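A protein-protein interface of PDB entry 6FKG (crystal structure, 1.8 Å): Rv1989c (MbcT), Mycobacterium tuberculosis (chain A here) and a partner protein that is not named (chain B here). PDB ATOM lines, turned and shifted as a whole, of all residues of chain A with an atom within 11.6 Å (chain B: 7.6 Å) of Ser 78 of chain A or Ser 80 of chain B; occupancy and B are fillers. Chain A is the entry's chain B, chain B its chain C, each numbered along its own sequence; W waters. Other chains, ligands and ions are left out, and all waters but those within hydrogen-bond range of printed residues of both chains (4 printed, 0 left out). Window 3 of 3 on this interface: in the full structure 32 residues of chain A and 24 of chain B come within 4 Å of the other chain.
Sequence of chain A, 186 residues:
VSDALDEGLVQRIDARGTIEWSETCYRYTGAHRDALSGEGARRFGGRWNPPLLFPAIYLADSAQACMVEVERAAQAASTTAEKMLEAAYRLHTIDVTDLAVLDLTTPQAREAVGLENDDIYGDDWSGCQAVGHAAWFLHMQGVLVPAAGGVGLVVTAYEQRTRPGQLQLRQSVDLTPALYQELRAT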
ATOM      1  N   TYR A  28      -9.435  19.869 -34.550  1.00  0.00           N
ATOM      2  CA  TYR A  28      -8.412  20.883 -34.291  1.00  0.00           C
ATOM      3  C   TYR A  28      -7.653  20.515 -33.012  1.00  0.00           C
ATOM      4  O   TYR A  28      -8.180  19.842 -32.118  1.00  0.00           O
ATOM      5  CB  TYR A  28      -9.023  22.316 -34.221  1.00  0.00           C
ATOM      6  CG  TYR A  28      -9.742  22.608 -32.924  1.00  0.00           C
ATOM      7  CD1 TYR A  28     -11.006  22.095 -32.682  1.00  0.00           C
ATOM      8  CD2 TYR A  28      -9.154  23.395 -31.942  1.00  0.00           C
ATOM      9  CE1 TYR A  28     -11.661  22.337 -31.494  1.00  0.00           C
ATOM     10  CE2 TYR A  28      -9.802  23.637 -30.740  1.00  0.00           C
ATOM     11  CZ  TYR A  28     -11.050  23.107 -30.524  1.00  0.00           C
ATOM     12  OH  TYR A  28     -11.698  23.356 -29.332  1.00  0.00           O
ATOM     13  N   GLU A  69     -17.303  24.140 -33.118  1.00  0.00           N
ATOM     14  CA  GLU A  69     -16.785  23.570 -31.870  1.00  0.00           C
ATOM     15  C   GLU A  69     -15.631  24.424 -31.320  1.00  0.00           C
ATOM     16  O   GLU A  69     -15.491  24.579 -30.101  1.00  0.00           O
ATOM     17  CB  GLU A  69     -16.346  22.118 -32.069  1.00  0.00           C
ATOM     18  CG  GLU A  69     -17.505  21.157 -32.425  1.00  0.00           C
ATOM     19  CD  GLU A  69     -18.633  21.162 -31.398  1.00  0.00           C
ATOM     20  OE1 GLU A  69     -18.376  21.336 -30.186  1.00  0.00           O
ATOM     21  OE2 GLU A  69     -19.794  20.998 -31.807  1.00  0.00           O
ATOM     22  N   VAL A  70     -14.844  25.029 -32.209  1.00  0.00           N
ATOM     23  CA  VAL A  70     -13.804  25.949 -31.755  1.00  0.00           C
ATOM     24  C   VAL A  70     -14.446  27.118 -30.990  1.00  0.00           C
ATOM     25  O   VAL A  70     -13.960  27.531 -29.944  1.00  0.00           O
ATOM     26  CB  VAL A  70     -12.941  26.495 -32.923  1.00  0.00           C
ATOM     27  CG1 VAL A  70     -11.961  27.557 -32.413  1.00  0.00           C
ATOM     28  CG2 VAL A  70     -12.168  25.362 -33.607  1.00  0.00           C
ATOM     29  N   GLU A  71     -15.561  27.628 -31.506  1.00  0.00           N
ATOM     30  CA  GLU A  71     -16.291  28.702 -30.832  1.00  0.00           C
ATOM     31  C   GLU A  71     -16.787  28.301 -29.444  1.00  0.00           C
ATOM     32  O   GLU A  71     -16.694  29.073 -28.486  1.00  0.00           O
ATOM     33  CB  GLU A  71     -17.502  29.136 -31.663  1.00  0.00           C
ATOM     34  CG  GLU A  71     -17.183  29.640 -33.025  1.00  0.00           C
ATOM     35  CD  GLU A  71     -18.448  30.063 -33.777  1.00  0.00           C
ATOM     36  OE1 GLU A  71     -19.567  29.922 -33.226  1.00  0.00           O
ATOM     37  OE2 GLU A  71     -18.320  30.533 -34.919  1.00  0.00           O
ATOM     38  N   ARG A  72     -17.378  27.112 -29.358  1.00  0.00           N
ATOM     39  CA  ARG A  72     -17.904  26.618 -28.090  1.00  0.00           C
ATOM     40  C   ARG A  72     -16.799  26.428 -27.058  1.00  0.00           C
ATOM     41  O   ARG A  72     -16.993  26.720 -25.882  1.00  0.00           O
ATOM     42  CB  ARG A  72     -18.658  25.304 -28.288  1.00  0.00           C
ATOM     43  CG  ARG A  72     -19.935  25.461 -29.129  1.00  0.00           C
ATOM     44  CD  ARG A  72     -20.650  24.116 -29.296  1.00  0.00           C
ATOM     45  NE  ARG A  72     -21.263  23.666 -28.050  1.00  0.00           N
ATOM     46  CZ  ARG A  72     -20.885  22.594 -27.369  1.00  0.00           C
ATOM     47  NH1 ARG A  72     -19.885  21.841 -27.816  1.00  0.00           N
ATOM     48  NH2 ARG A  72     -21.519  22.277 -26.239  1.00  0.00           N
ATOM     49  N   ALA A  73     -15.646  25.926 -27.489  1.00  0.00           N
ATOM     50  CA  ALA A  73     -14.531  25.808 -26.566  1.00  0.00           C
ATOM     51  C   ALA A  73     -14.042  27.186 -26.130  1.00  0.00           C
ATOM     52  O   ALA A  73     -13.779  27.419 -24.947  1.00  0.00           O
ATOM     53  CB  ALA A  73     -13.393  24.998 -27.202  1.00  0.00           C
ATOM     54  N   ALA A  74     -13.918  28.104 -27.083  1.00  0.00           N
ATOM     55  CA  ALA A  74     -13.535  29.471 -26.757  1.00  0.00           C
ATOM     56  C   ALA A  74     -14.467  30.091 -25.730  1.00  0.00           C
ATOM     57  O   ALA A  74     -14.023  30.750 -24.793  1.00  0.00           O
ATOM     58  CB  ALA A  74     -13.509  30.330 -28.023  1.00  0.00           C
ATOM     59  N   GLN A  75     -15.768  29.902 -25.928  1.00  0.00           N
ATOM     60  CA  GLN A  75     -16.768  30.427 -25.022  1.00  0.00           C
ATOM     61  C   GLN A  75     -16.629  29.834 -23.610  1.00  0.00           C
ATOM     62  O   GLN A  75     -16.753  30.553 -22.625  1.00  0.00           O
ATOM     63  CB  GLN A  75     -18.185  30.170 -25.584  1.00  0.00           C
ATOM     64  CG  GLN A  75     -19.305  30.718 -24.725  1.00  0.00           C
ATOM     65  CD  GLN A  75     -20.673  30.166 -25.122  1.00  0.00           C
ATOM     66  OE1 GLN A  75     -20.792  29.379 -26.068  1.00  0.00           O
ATOM     67  NE2 GLN A  75     -21.714  30.589 -24.407  1.00  0.00           N
ATOM     68  N   ALA A  76     -16.354  28.538 -23.505  1.00  0.00           N
ATOM     69  CA  ALA A  76     -16.144  27.905 -22.195  1.00  0.00           C
ATOM     70  C   ALA A  76     -14.876  28.442 -21.538  1.00  0.00           C
ATOM     71  O   ALA A  76     -14.730  28.395 -20.314  1.00  0.00           O
ATOM     72  CB  ALA A  76     -16.063  26.370 -22.329  1.00  0.00           C
ATOM     73  N   ALA A  77     -13.966  28.944 -22.370  1.00  0.00           N
ATOM     74  CA  ALA A  77     -12.721  29.553 -21.917  1.00  0.00           C
ATOM     75  C   ALA A  77     -12.872  31.071 -21.758  1.00  0.00           C
ATOM     76  O   ALA A  77     -11.880  31.776 -21.648  1.00  0.00           O
ATOM     77  CB  ALA A  77     -11.600  29.237 -22.892  1.00  0.00           C
ATOM     78  N   SER A  78     -14.112  31.559 -21.758  1.00  0.00           N
ATOM     79  CA  SER A  78     -14.411  32.979 -21.525  1.00  0.00           C
ATOM     80  C   SER A  78     -13.826  33.917 -22.589  1.00  0.00           C
ATOM     81  O   SER A  78     -13.546  35.093 -22.320  1.00  0.00           O
ATOM     82  CB  SER A  78     -13.906  33.412 -20.137  1.00  0.00           C
ATOM     83  OG  SER A  78     -14.563  32.688 -19.108  1.00  0.00           O
ATOM     84  N   THR A  79     -13.642  33.415 -23.799  1.00  0.00           N
ATOM     85  CA  THR A  79     -13.121  34.265 -24.851  1.00  0.00           C
ATOM     86  C   THR A  79     -13.810  33.929 -26.182  1.00  0.00           C
ATOM     87  O   THR A  79     -14.921  33.399 -26.184  1.00  0.00           O
ATOM     88  CB  THR A  79     -11.584  34.148 -24.953  1.00  0.00           C
ATOM     89  OG1 THR A  79     -11.096  35.095 -25.910  1.00  0.00           O
ATOM     90  CG2 THR A  79     -11.130  32.709 -25.317  1.00  0.00           C
ATOM     91  N   THR A  80     -13.178  34.273 -27.302  1.00  0.00           N
ATOM     92  CA  THR A  80     -13.765  34.034 -28.620  1.00  0.00           C
ATOM     93  C   THR A  80     -12.805  33.229 -29.469  1.00  0.00           C
ATOM     94  O   THR A  80     -11.607  33.194 -29.177  1.00  0.00           O
ATOM     95  CB  THR A  80     -14.077  35.329 -29.358  1.00  0.00           C
ATOM     96  OG1 THR A  80     -12.854  36.039 -29.596  1.00  0.00           O
ATOM     97  CG2 THR A  80     -15.034  36.205 -28.552  1.00  0.00           C
ATOM     98  N   ALA A  81     -13.322  32.586 -30.514  1.00  0.00           N
ATOM     99  CA  ALA A  81     -12.474  31.806 -31.419  1.00  0.00           C
ATOM    100  C   ALA A  81     -11.355  32.694 -31.972  1.00  0.00           C
ATOM    101  O   ALA A  81     -10.199  32.275 -32.013  1.00  0.00           O
ATOM    102  CB  ALA A  81     -13.298  31.201 -32.566  1.00  0.00           C
ATOM    103  N   GLU A  82     -11.709  33.916 -32.377  1.00  0.00           N
ATOM    104  CA  GLU A  82     -10.747  34.866 -32.933  1.00  0.00           C
ATOM    105  C   GLU A  82      -9.559  35.129 -32.023  1.00  0.00           C
ATOM    106  O   GLU A  82      -8.426  35.216 -32.489  1.00  0.00           O
ATOM    107  CB  GLU A  82     -11.426  36.203 -33.235  1.00  0.00           C
ATOM    108  CG  GLU A  82     -12.281  36.208 -34.477  1.00  0.00           C
ATOM    109  CD  GLU A  82     -13.686  35.695 -34.234  1.00  0.00           C
ATOM    110  OE1 GLU A  82     -13.997  35.246 -33.101  1.00  0.00           O
ATOM    111  OE2 GLU A  82     -14.492  35.771 -35.187  1.00  0.00           O
ATOM    112  N   LYS A  83      -9.816  35.270 -30.730  1.00  0.00           N
ATOM    113  CA  LYS A  83      -8.744  35.526 -29.764  1.00  0.00           C
ATOM    114  C   LYS A  83      -8.005  34.249 -29.365  1.00  0.00           C
ATOM    115  O   LYS A  83      -6.783  34.246 -29.216  1.00  0.00           O
ATOM    116  CB  LYS A  83      -9.304  36.201 -28.513  1.00  0.00           C
ATOM    117  CG  LYS A  83      -9.752  37.649 -28.712  1.00  0.00           C
ATOM    118  CD  LYS A  83      -8.566  38.571 -28.978  1.00  0.00           C
ATOM    119  CE  LYS A  83      -8.985  40.027 -29.058  1.00  0.00           C
ATOM    120  NZ  LYS A  83      -7.860  40.895 -29.518  1.00  0.00           N
ATOM    121  N   MET A  84      -8.749  33.163 -29.178  1.00  0.00           N
ATOM    122  CA  MET A  84      -8.146  31.889 -28.764  1.00  0.00           C
ATOM    123  C   MET A  84      -7.133  31.404 -29.787  1.00  0.00           C
ATOM    124  O   MET A  84      -6.065  30.867 -29.432  1.00  0.00           O
ATOM    125  CB  MET A  84      -9.227  30.824 -28.553  1.00  0.00           C
ATOM    126  CG  MET A  84      -8.707  29.475 -28.059  1.00  0.00           C
ATOM    127  SD  MET A  84     -10.082  28.356 -27.693  1.00  0.00           S
ATOM    128  CE  MET A  84     -10.266  27.530 -29.255  1.00  0.00           C
ATOM    129  N   LEU A  85      -7.465  31.606 -31.060  1.00  0.00           N
ATOM    130  CA  LEU A  85      -6.627  31.118 -32.155  1.00  0.00           C
ATOM    131  C   LEU A  85      -5.392  31.987 -32.400  1.00  0.00           C
ATOM    132  O   LEU A  85      -4.651  31.767 -33.354  1.00  0.00           O
ATOM    133  CB  LEU A  85      -7.448  31.011 -33.427  1.00  0.00           C
ATOM    134  CG  LEU A  85      -8.504  29.903 -33.380  1.00  0.00           C
ATOM    135  CD1 LEU A  85      -9.376  29.974 -34.618  1.00  0.00           C
ATOM    136  CD2 LEU A  85      -7.835  28.508 -33.256  1.00  0.00           C
ATOM    137  N   TYR A  89      -2.845  26.871 -33.076  1.00  0.00           N
ATOM    138  CA  TYR A  89      -3.645  25.670 -33.320  1.00  0.00           C
ATOM    139  C   TYR A  89      -3.518  25.222 -34.771  1.00  0.00           C
ATOM    140  O   TYR A  89      -3.158  26.005 -35.654  1.00  0.00           O
ATOM    141  CB  TYR A  89      -5.126  25.910 -33.017  1.00  0.00           C
ATOM    142  CG  TYR A  89      -5.462  26.057 -31.554  1.00  0.00           C
ATOM    143  CD1 TYR A  89      -5.375  27.292 -30.923  1.00  0.00           C
ATOM    144  CD2 TYR A  89      -5.879  24.959 -30.810  1.00  0.00           C
ATOM    145  CE1 TYR A  89      -5.700  27.426 -29.568  1.00  0.00           C
ATOM    146  CE2 TYR A  89      -6.193  25.072 -29.457  1.00  0.00           C
ATOM    147  CZ  TYR A  89      -6.117  26.313 -28.848  1.00  0.00           C
ATOM    148  OH  TYR A  89      -6.437  26.434 -27.515  1.00  0.00           O
ATOM    149  N   LEU B  69      -3.945  29.371 -24.785  1.00  0.00           N
ATOM    150  CA  LEU B  69      -4.491  30.743 -24.806  1.00  0.00           C
ATOM    151  C   LEU B  69      -3.403  31.794 -24.825  1.00  0.00           C
ATOM    152  O   LEU B  69      -2.402  31.656 -24.137  1.00  0.00           O
ATOM    153  CB  LEU B  69      -5.375  31.010 -23.596  1.00  0.00           C
ATOM    154  CG  LEU B  69      -6.708  30.285 -23.518  1.00  0.00           C
ATOM    155  CD1 LEU B  69      -7.291  30.550 -22.139  1.00  0.00           C
ATOM    156  CD2 LEU B  69      -7.645  30.756 -24.646  1.00  0.00           C
ATOM    157  N   GLN B  73      -5.840  36.587 -22.504  1.00  0.00           N
ATOM    158  CA  GLN B  73      -6.968  35.689 -22.277  1.00  0.00           C
ATOM    159  C   GLN B  73      -6.625  34.609 -21.258  1.00  0.00           C
ATOM    160  O   GLN B  73      -7.480  34.153 -20.509  1.00  0.00           O
ATOM    161  CB  GLN B  73      -7.428  35.057 -23.599  1.00  0.00           C
ATOM    162  CG  GLN B  73      -8.297  36.021 -24.458  1.00  0.00           C
ATOM    163  CD  GLN B  73      -7.501  37.165 -25.057  1.00  0.00           C
ATOM    164  OE1 GLN B  73      -6.399  36.963 -25.559  1.00  0.00           O
ATOM    165  NE2 GLN B  73      -8.065  38.380 -25.017  1.00  0.00           N
ATOM    166  N   ALA B  74      -5.358  34.209 -21.225  1.00  0.00           N
ATOM    167  CA  ALA B  74      -4.904  33.231 -20.255  1.00  0.00           C
ATOM    168  C   ALA B  74      -5.085  33.807 -18.860  1.00  0.00           C
ATOM    169  O   ALA B  74      -5.582  33.150 -17.948  1.00  0.00           O
ATOM    170  CB  ALA B  74      -3.445  32.866 -20.510  1.00  0.00           C
ATOM    171  N   ASN B  75      -4.715  35.071 -18.718  1.00  0.00           N
ATOM    172  CA  ASN B  75      -4.847  35.749 -17.445  1.00  0.00           C
ATOM    173  C   ASN B  75      -6.309  35.802 -16.967  1.00  0.00           C
ATOM    174  O   ASN B  75      -6.617  35.411 -15.849  1.00  0.00           O
ATOM    175  CB  ASN B  75      -4.264  37.151 -17.568  1.00  0.00           C
ATOM    176  CG  ASN B  75      -4.294  37.904 -16.266  1.00  0.00           C
ATOM    177  OD1 ASN B  75      -5.354  38.302 -15.794  1.00  0.00           O
ATOM    178  ND2 ASN B  75      -3.121  38.136 -15.693  1.00  0.00           N
ATOM    179  N   VAL B  76      -7.199  36.294 -17.822  1.00  0.00           N
ATOM    180  CA  VAL B  76      -8.630  36.315 -17.519  1.00  0.00           C
ATOM    181  C   VAL B  76      -9.164  34.919 -17.169  1.00  0.00           C
ATOM    182  O   VAL B  76      -9.961  34.741 -16.243  1.00  0.00           O
ATOM    183  CB  VAL B  76      -9.435  36.866 -18.715  1.00  0.00           C
ATOM    184  CG1 VAL B  76     -10.938  36.749 -18.463  1.00  0.00           C
ATOM    185  CG2 VAL B  76      -9.025  38.323 -19.023  1.00  0.00           C
ATOM    186  N   TRP B  77      -8.737  33.932 -17.938  1.00  0.00           N
ATOM    187  CA  TRP B  77      -9.188  32.541 -17.743  1.00  0.00           C
ATOM    188  C   TRP B  77      -8.912  32.011 -16.336  1.00  0.00           C
ATOM    189  O   TRP B  77      -9.729  31.279 -15.763  1.00  0.00           O
ATOM    190  CB  TRP B  77      -8.497  31.648 -18.772  1.00  0.00           C
ATOM    191  CG  TRP B  77      -8.919  30.224 -18.812  1.00  0.00           C
ATOM    192  CD1 TRP B  77      -9.945  29.692 -19.551  1.00  0.00           C
ATOM    193  CD2 TRP B  77      -8.280  29.118 -18.147  1.00  0.00           C
ATOM    194  NE1 TRP B  77      -9.992  28.319 -19.364  1.00  0.00           N
ATOM    195  CE2 TRP B  77      -8.987  27.950 -18.504  1.00  0.00           C
ATOM    196  CE3 TRP B  77      -7.201  29.010 -17.260  1.00  0.00           C
ATOM    197  CZ2 TRP B  77      -8.640  26.683 -18.020  1.00  0.00           C
ATOM    198  CZ3 TRP B  77      -6.850  27.745 -16.784  1.00  0.00           C
ATOM    199  CH2 TRP B  77      -7.565  26.604 -17.169  1.00  0.00           C
ATOM    200  N   MET B  78      -7.768  32.394 -15.772  1.00  0.00           N
ATOM    201  CA  MET B  78      -7.403  31.939 -14.431  1.00  0.00           C
ATOM    202  C   MET B  78      -8.433  32.385 -13.406  1.00  0.00           C
ATOM    203  O   MET B  78      -8.654  31.678 -12.422  1.00  0.00           O
ATOM    204  CB  MET B  78      -6.019  32.461 -14.022  1.00  0.00           C
ATOM    205  CG  MET B  78      -4.870  31.854 -14.787  1.00  0.00           C
ATOM    206  SD  MET B  78      -4.613  30.122 -14.375  1.00  0.00           S
ATOM    207  CE  MET B  78      -4.175  30.238 -12.647  1.00  0.00           C
ATOM    208  N   PHE B  79      -9.092  33.526 -13.648  1.00  0.00           N
ATOM    209  CA  PHE B  79      -9.993  34.084 -12.637  1.00  0.00           C
ATOM    210  C   PHE B  79     -11.457  34.063 -13.054  1.00  0.00           C
ATOM    211  O   PHE B  79     -12.310  34.689 -12.420  1.00  0.00           O
ATOM    212  CB  PHE B  79      -9.543  35.509 -12.286  1.00  0.00           C
ATOM    213  CG  PHE B  79      -8.102  35.567 -11.877  1.00  0.00           C
ATOM    214  CD1 PHE B  79      -7.711  35.093 -10.635  1.00  0.00           C
ATOM    215  CD2 PHE B  79      -7.129  36.031 -12.754  1.00  0.00           C
ATOM    216  CE1 PHE B  79      -6.382  35.100 -10.264  1.00  0.00           C
ATOM    217  CE2 PHE B  79      -5.799  36.048 -12.388  1.00  0.00           C
ATOM    218  CZ  PHE B  79      -5.421  35.580 -11.144  1.00  0.00           C
ATOM    219  N   SER B  80     -11.751  33.312 -14.108  1.00  0.00           N
ATOM    220  CA  SER B  80     -13.115  33.211 -14.600  1.00  0.00           C
ATOM    221  C   SER B  80     -13.737  31.906 -14.161  1.00  0.00           C
ATOM    222  O   SER B  80     -13.161  30.840 -14.395  1.00  0.00           O
ATOM    223  CB  SER B  80     -13.152  33.308 -16.122  1.00  0.00           C
ATOM    224  OG  SER B  80     -12.622  34.544 -16.568  1.00  0.00           O
ATOM    225  N   PRO B  81     -14.918  31.985 -13.529  1.00  0.00           N
ATOM    226  CA  PRO B  81     -15.703  30.785 -13.238  1.00  0.00           C
ATOM    227  C   PRO B  81     -15.871  29.987 -14.513  1.00  0.00           C
ATOM    228  O   PRO B  81     -16.293  30.515 -15.538  1.00  0.00           O
ATOM    229  CB  PRO B  81     -17.038  31.344 -12.735  1.00  0.00           C
ATOM    230  CG  PRO B  81     -16.677  32.682 -12.154  1.00  0.00           C
ATOM    231  CD  PRO B  81     -15.596  33.215 -13.070  1.00  0.00           C
ATOM    232  N   ASN B  82     -15.495  28.723 -14.454  1.00  0.00           N
ATOM    233  CA  ASN B  82     -15.422  27.892 -15.641  1.00  0.00           C
ATOM    234  C   ASN B  82     -16.435  26.760 -15.516  1.00  0.00           C
ATOM    235  O   ASN B  82     -16.348  25.949 -14.585  1.00  0.00           O
ATOM    236  CB  ASN B  82     -13.990  27.352 -15.801  1.00  0.00           C
ATOM    237  CG  ASN B  82     -13.735  26.734 -17.162  1.00  0.00           C
ATOM    238  OD1 ASN B  82     -14.519  25.931 -17.645  1.00  0.00           O
ATOM    239  ND2 ASN B  82     -12.636  27.132 -17.794  1.00  0.00           N
ATOM    240  N   ARG B  83     -17.387  26.693 -16.442  1.00  0.00           N
ATOM    241  CA  ARG B  83     -18.434  25.668 -16.357  1.00  0.00           C
ATOM    242  C   ARG B  83     -17.877  24.237 -16.469  1.00  0.00           C
ATOM    243  O   ARG B  83     -18.522  23.285 -16.028  1.00  0.00           O
ATOM    244  CB  ARG B  83     -19.518  25.897 -17.426  1.00  0.00           C
ATOM    245  CG  ARG B  83     -19.085  25.687 -18.875  1.00  0.00           C
ATOM    246  CD  ARG B  83     -20.331  25.531 -19.771  1.00  0.00           C
ATOM    247  NE  ARG B  83     -20.006  25.412 -21.189  1.00  0.00           N
ATOM    248  CZ  ARG B  83     -19.830  24.256 -21.833  1.00  0.00           C
ATOM    249  NH1 ARG B  83     -19.938  23.093 -21.196  1.00  0.00           N
ATOM    250  NH2 ARG B  83     -19.540  24.259 -23.127  1.00  0.00           N
ATOM    251  N   LEU B  85     -15.325  23.261 -14.883  1.00  0.00           N
ATOM    252  CA  LEU B  85     -14.817  22.968 -13.548  1.00  0.00           C
ATOM    253  C   LEU B  85     -15.896  23.229 -12.500  1.00  0.00           C
ATOM    254  O   LEU B  85     -15.609  23.731 -11.418  1.00  0.00           O
ATOM    255  CB  LEU B  85     -13.566  23.813 -13.252  1.00  0.00           C
ATOM    256  CG  LEU B  85     -12.387  23.700 -14.220  1.00  0.00           C
ATOM    257  CD1 LEU B  85     -11.337  24.728 -13.847  1.00  0.00           C
ATOM    258  CD2 LEU B  85     -11.767  22.285 -14.220  1.00  0.00           C
ATOM    259  N   HIS B  87     -18.106  25.473 -12.445  1.00  0.00           N
ATOM    260  CA  HIS B  87     -18.256  26.912 -12.248  1.00  0.00           C
ATOM    261  C   HIS B  87     -17.288  27.448 -11.204  1.00  0.00           C
ATOM    262  O   HIS B  87     -17.594  28.406 -10.509  1.00  0.00           O
ATOM    263  CB  HIS B  87     -19.705  27.256 -11.865  1.00  0.00           C
ATOM    264  CG  HIS B  87     -20.719  26.710 -12.822  1.00  0.00           C
ATOM    265  ND1 HIS B  87     -20.907  27.231 -14.083  1.00  0.00           N
ATOM    266  CD2 HIS B  87     -21.583  25.672 -12.711  1.00  0.00           C
ATOM    267  CE1 HIS B  87     -21.852  26.548 -14.704  1.00  0.00           C
ATOM    268  NE2 HIS B  87     -22.282  25.599 -13.891  1.00  0.00           N
ATOM    269  N   ARG B  88     -16.118  26.819 -11.098  1.00  0.00           N
ATOM    270  CA  ARG B  88     -15.062  27.306 -10.221  1.00  0.00           C
ATOM    271  C   ARG B  88     -13.960  27.969 -11.047  1.00  0.00           C
ATOM    272  O   ARG B  88     -13.836  27.719 -12.239  1.00  0.00           O
ATOM    273  CB  ARG B  88     -14.490  26.157  -9.375  1.00  0.00           C
ATOM    274  CG  ARG B  88     -15.480  25.591  -8.361  1.00  0.00           C
ATOM    275  CD  ARG B  88     -14.899  24.372  -7.643  1.00  0.00           C
ATOM    276  NE  ARG B  88     -14.690  23.268  -8.578  1.00  0.00           N
ATOM    277  CZ  ARG B  88     -13.834  22.268  -8.384  1.00  0.00           C
ATOM    278  NH1 ARG B  88     -13.091  22.224  -7.283  1.00  0.00           N
ATOM    279  NH2 ARG B  88     -13.717  21.309  -9.299  1.00  0.00           N
ATOM    280  N   LYS B  89     -13.177  28.836 -10.411  1.00  0.00           N
ATOM    281  CA  LYS B  89     -12.053  29.494 -11.072  1.00  0.00           C
ATOM    282  C   LYS B  89     -10.821  28.593 -11.039  1.00  0.00           C
ATOM    283  O   LYS B  89     -10.499  28.047  -9.980  1.00  0.00           O
ATOM    284  CB  LYS B  89     -11.715  30.816 -10.386  1.00  0.00           C
ATOM    285  CG  LYS B  89     -12.840  31.858 -10.363  1.00  0.00           C
ATOM    286  CD  LYS B  89     -12.474  32.997  -9.431  1.00  0.00           C
ATOM    287  CE  LYS B  89     -13.671  33.905  -9.184  1.00  0.00           C
ATOM    288  NZ  LYS B  89     -13.335  35.080  -8.337  1.00  0.00           N
ATOM    289  N   PRO B  90     -10.118  28.452 -12.179  1.00  0.00           N
ATOM    290  CA  PRO B  90      -8.859  27.680 -12.159  1.00  0.00           C
ATOM    291  C   PRO B  90      -7.876  28.125 -11.063  1.00  0.00           C
ATOM    292  O   PRO B  90      -7.230  27.270 -10.447  1.00  0.00           O
ATOM    293  CB  PRO B  90      -8.270  27.939 -13.553  1.00  0.00           C
ATOM    294  CG  PRO B  90      -9.508  28.182 -14.429  1.00  0.00           C
ATOM    295  CD  PRO B  90     -10.502  28.873 -13.545  1.00  0.00           C
ATOM    296  N   ALA B  91      -7.765  29.430 -10.821  1.00  0.00           N
ATOM    297  CA  ALA B  91      -6.869  29.928  -9.774  1.00  0.00           C
ATOM    298  C   ALA B  91      -7.242  29.393  -8.388  1.00  0.00           C
ATOM    299  O   ALA B  91      -6.364  29.111  -7.572  1.00  0.00           O
ATOM    300  CB  ALA B  91      -6.854  31.457  -9.761  1.00  0.00           C
HETATM  301  O   HOH W   1      -6.375  40.321 -26.697  1.00  0.00           O
HETATM  302  O   HOH W   2     -19.453  26.664 -24.634  1.00  0.00           O
HETATM  303  O   HOH W   3     -11.226  37.541 -25.005  1.00  0.00           O
HETATM  304  O   HOH W   4     -10.157  34.227 -21.499  1.00  0.00           O
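OG of Ser 80 of chain B lies within hydrogen-bond range of O of Val 76 of chain B, 2.7 Å away. N of Thr 79 of chain A lies within hydrogen-bond range of O of Ala 74 of chain A (2.9 Å). The indole nitrogen (NE1) of Trp 77 of chain B sits close to the side-chain amide nitrogen (ND2) of Asn 82 of chain B (3.3 Å). The backbone NH (N) of Asn 82 of chain B lies within hydrogen-bond range of the backbone carbonyl oxygen (O) of Arg 88 of chain B (2.9 Å). N of Lys 83 of chain A lies within hydrogen-bond range of OG1 of Thr 80 of chain A, 3.3 Å away. O of Asn 82 of chain B lies within hydrogen-bond range of N of His 87 of chain B, at 2.8 Å.
Water W3 lies within hydrogen-bond range of OG1 of Thr 79 of chain A and NE2 of Gln 73 of chain B. Water W2 lies within hydrogen-bond range of O of Arg 72 of chain A, NH2 of Arg 83 of chain B and OE1 of Gln 75 of chain A. Water W4 bridges O of Gln 73 of chain B (2.9 Å) and O of Ala 77 of chain A (3.0 Å). Water W1 bridges the side-chain amide nitrogen of Gln 73 of chain B (3.1 Å) and the side-chain amino group of Lys 83 of chain A (3.2 Å).
Asn 82 of chain B touches Ala 76 of chain A. Trp 77 of chain B touches Ala 77 of chain A. Ser 78 of chain A touches Ser 80 of chain B. Thr 79 of chain A touches Gln 73 of chain B (OG1 to CG, 3.3 Å). Lys 83 of chain A touches Gln 73 of chain B. Leu 69 of chain B touches Met 84 of chain A.
Of the 19 printed residues of chain A, 6 touch a printed residue of chain B. Hydrophobic or aromatic side chains of chain A within 4 Å of the printed part of chain B: Ala 77 and Met 84. Printed residues of chain B that touch a printed residue of chain A: Leu 69, Gln 73, Trp 77, Ser 80 and Asn 82. Among the printed residues, 6 pairs touch across the chains. Among the printed residues, no Asp or Glu carboxylate lies within 4 Å of a Lys or Arg side-chain nitrogen of the other chain.
Of the printed residues of chain B, Ser 78 of chain A touches Ser 80. Of chain A, only Ser 78 (3.4 Å) comes within 4 Å of Ser 80 of chain B. Val 76 of chain B touches none of the printed residues of chain A. Of the printed residues of chain A, Trp 77 of chain B touches Ala 77 (3.5 Å). No residue of chain A comes within 4 Å of Phe 79 of chain B. No residue of chain A comes within 4 Å of Pro 81 of chain B. Asn 82 of chain B touches one residue of chain A. No residue of chain A comes within 4 Å of Lys 89 of chain B. Of the printed residues of chain B, Met 84 of chain A touches Leu 69. Of the printed residues of chain A, Leu 69 of chain B touches Met 84. Printed residues of chain B within 4 Å of Ala 76 of chain A: Asn 82. Of the printed residues of chain A, Gln 73 of chain B touches Thr 79 and Lys 83. Printed residues of chain B within 4 Å of Ala 77 of chain A: Trp 77.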
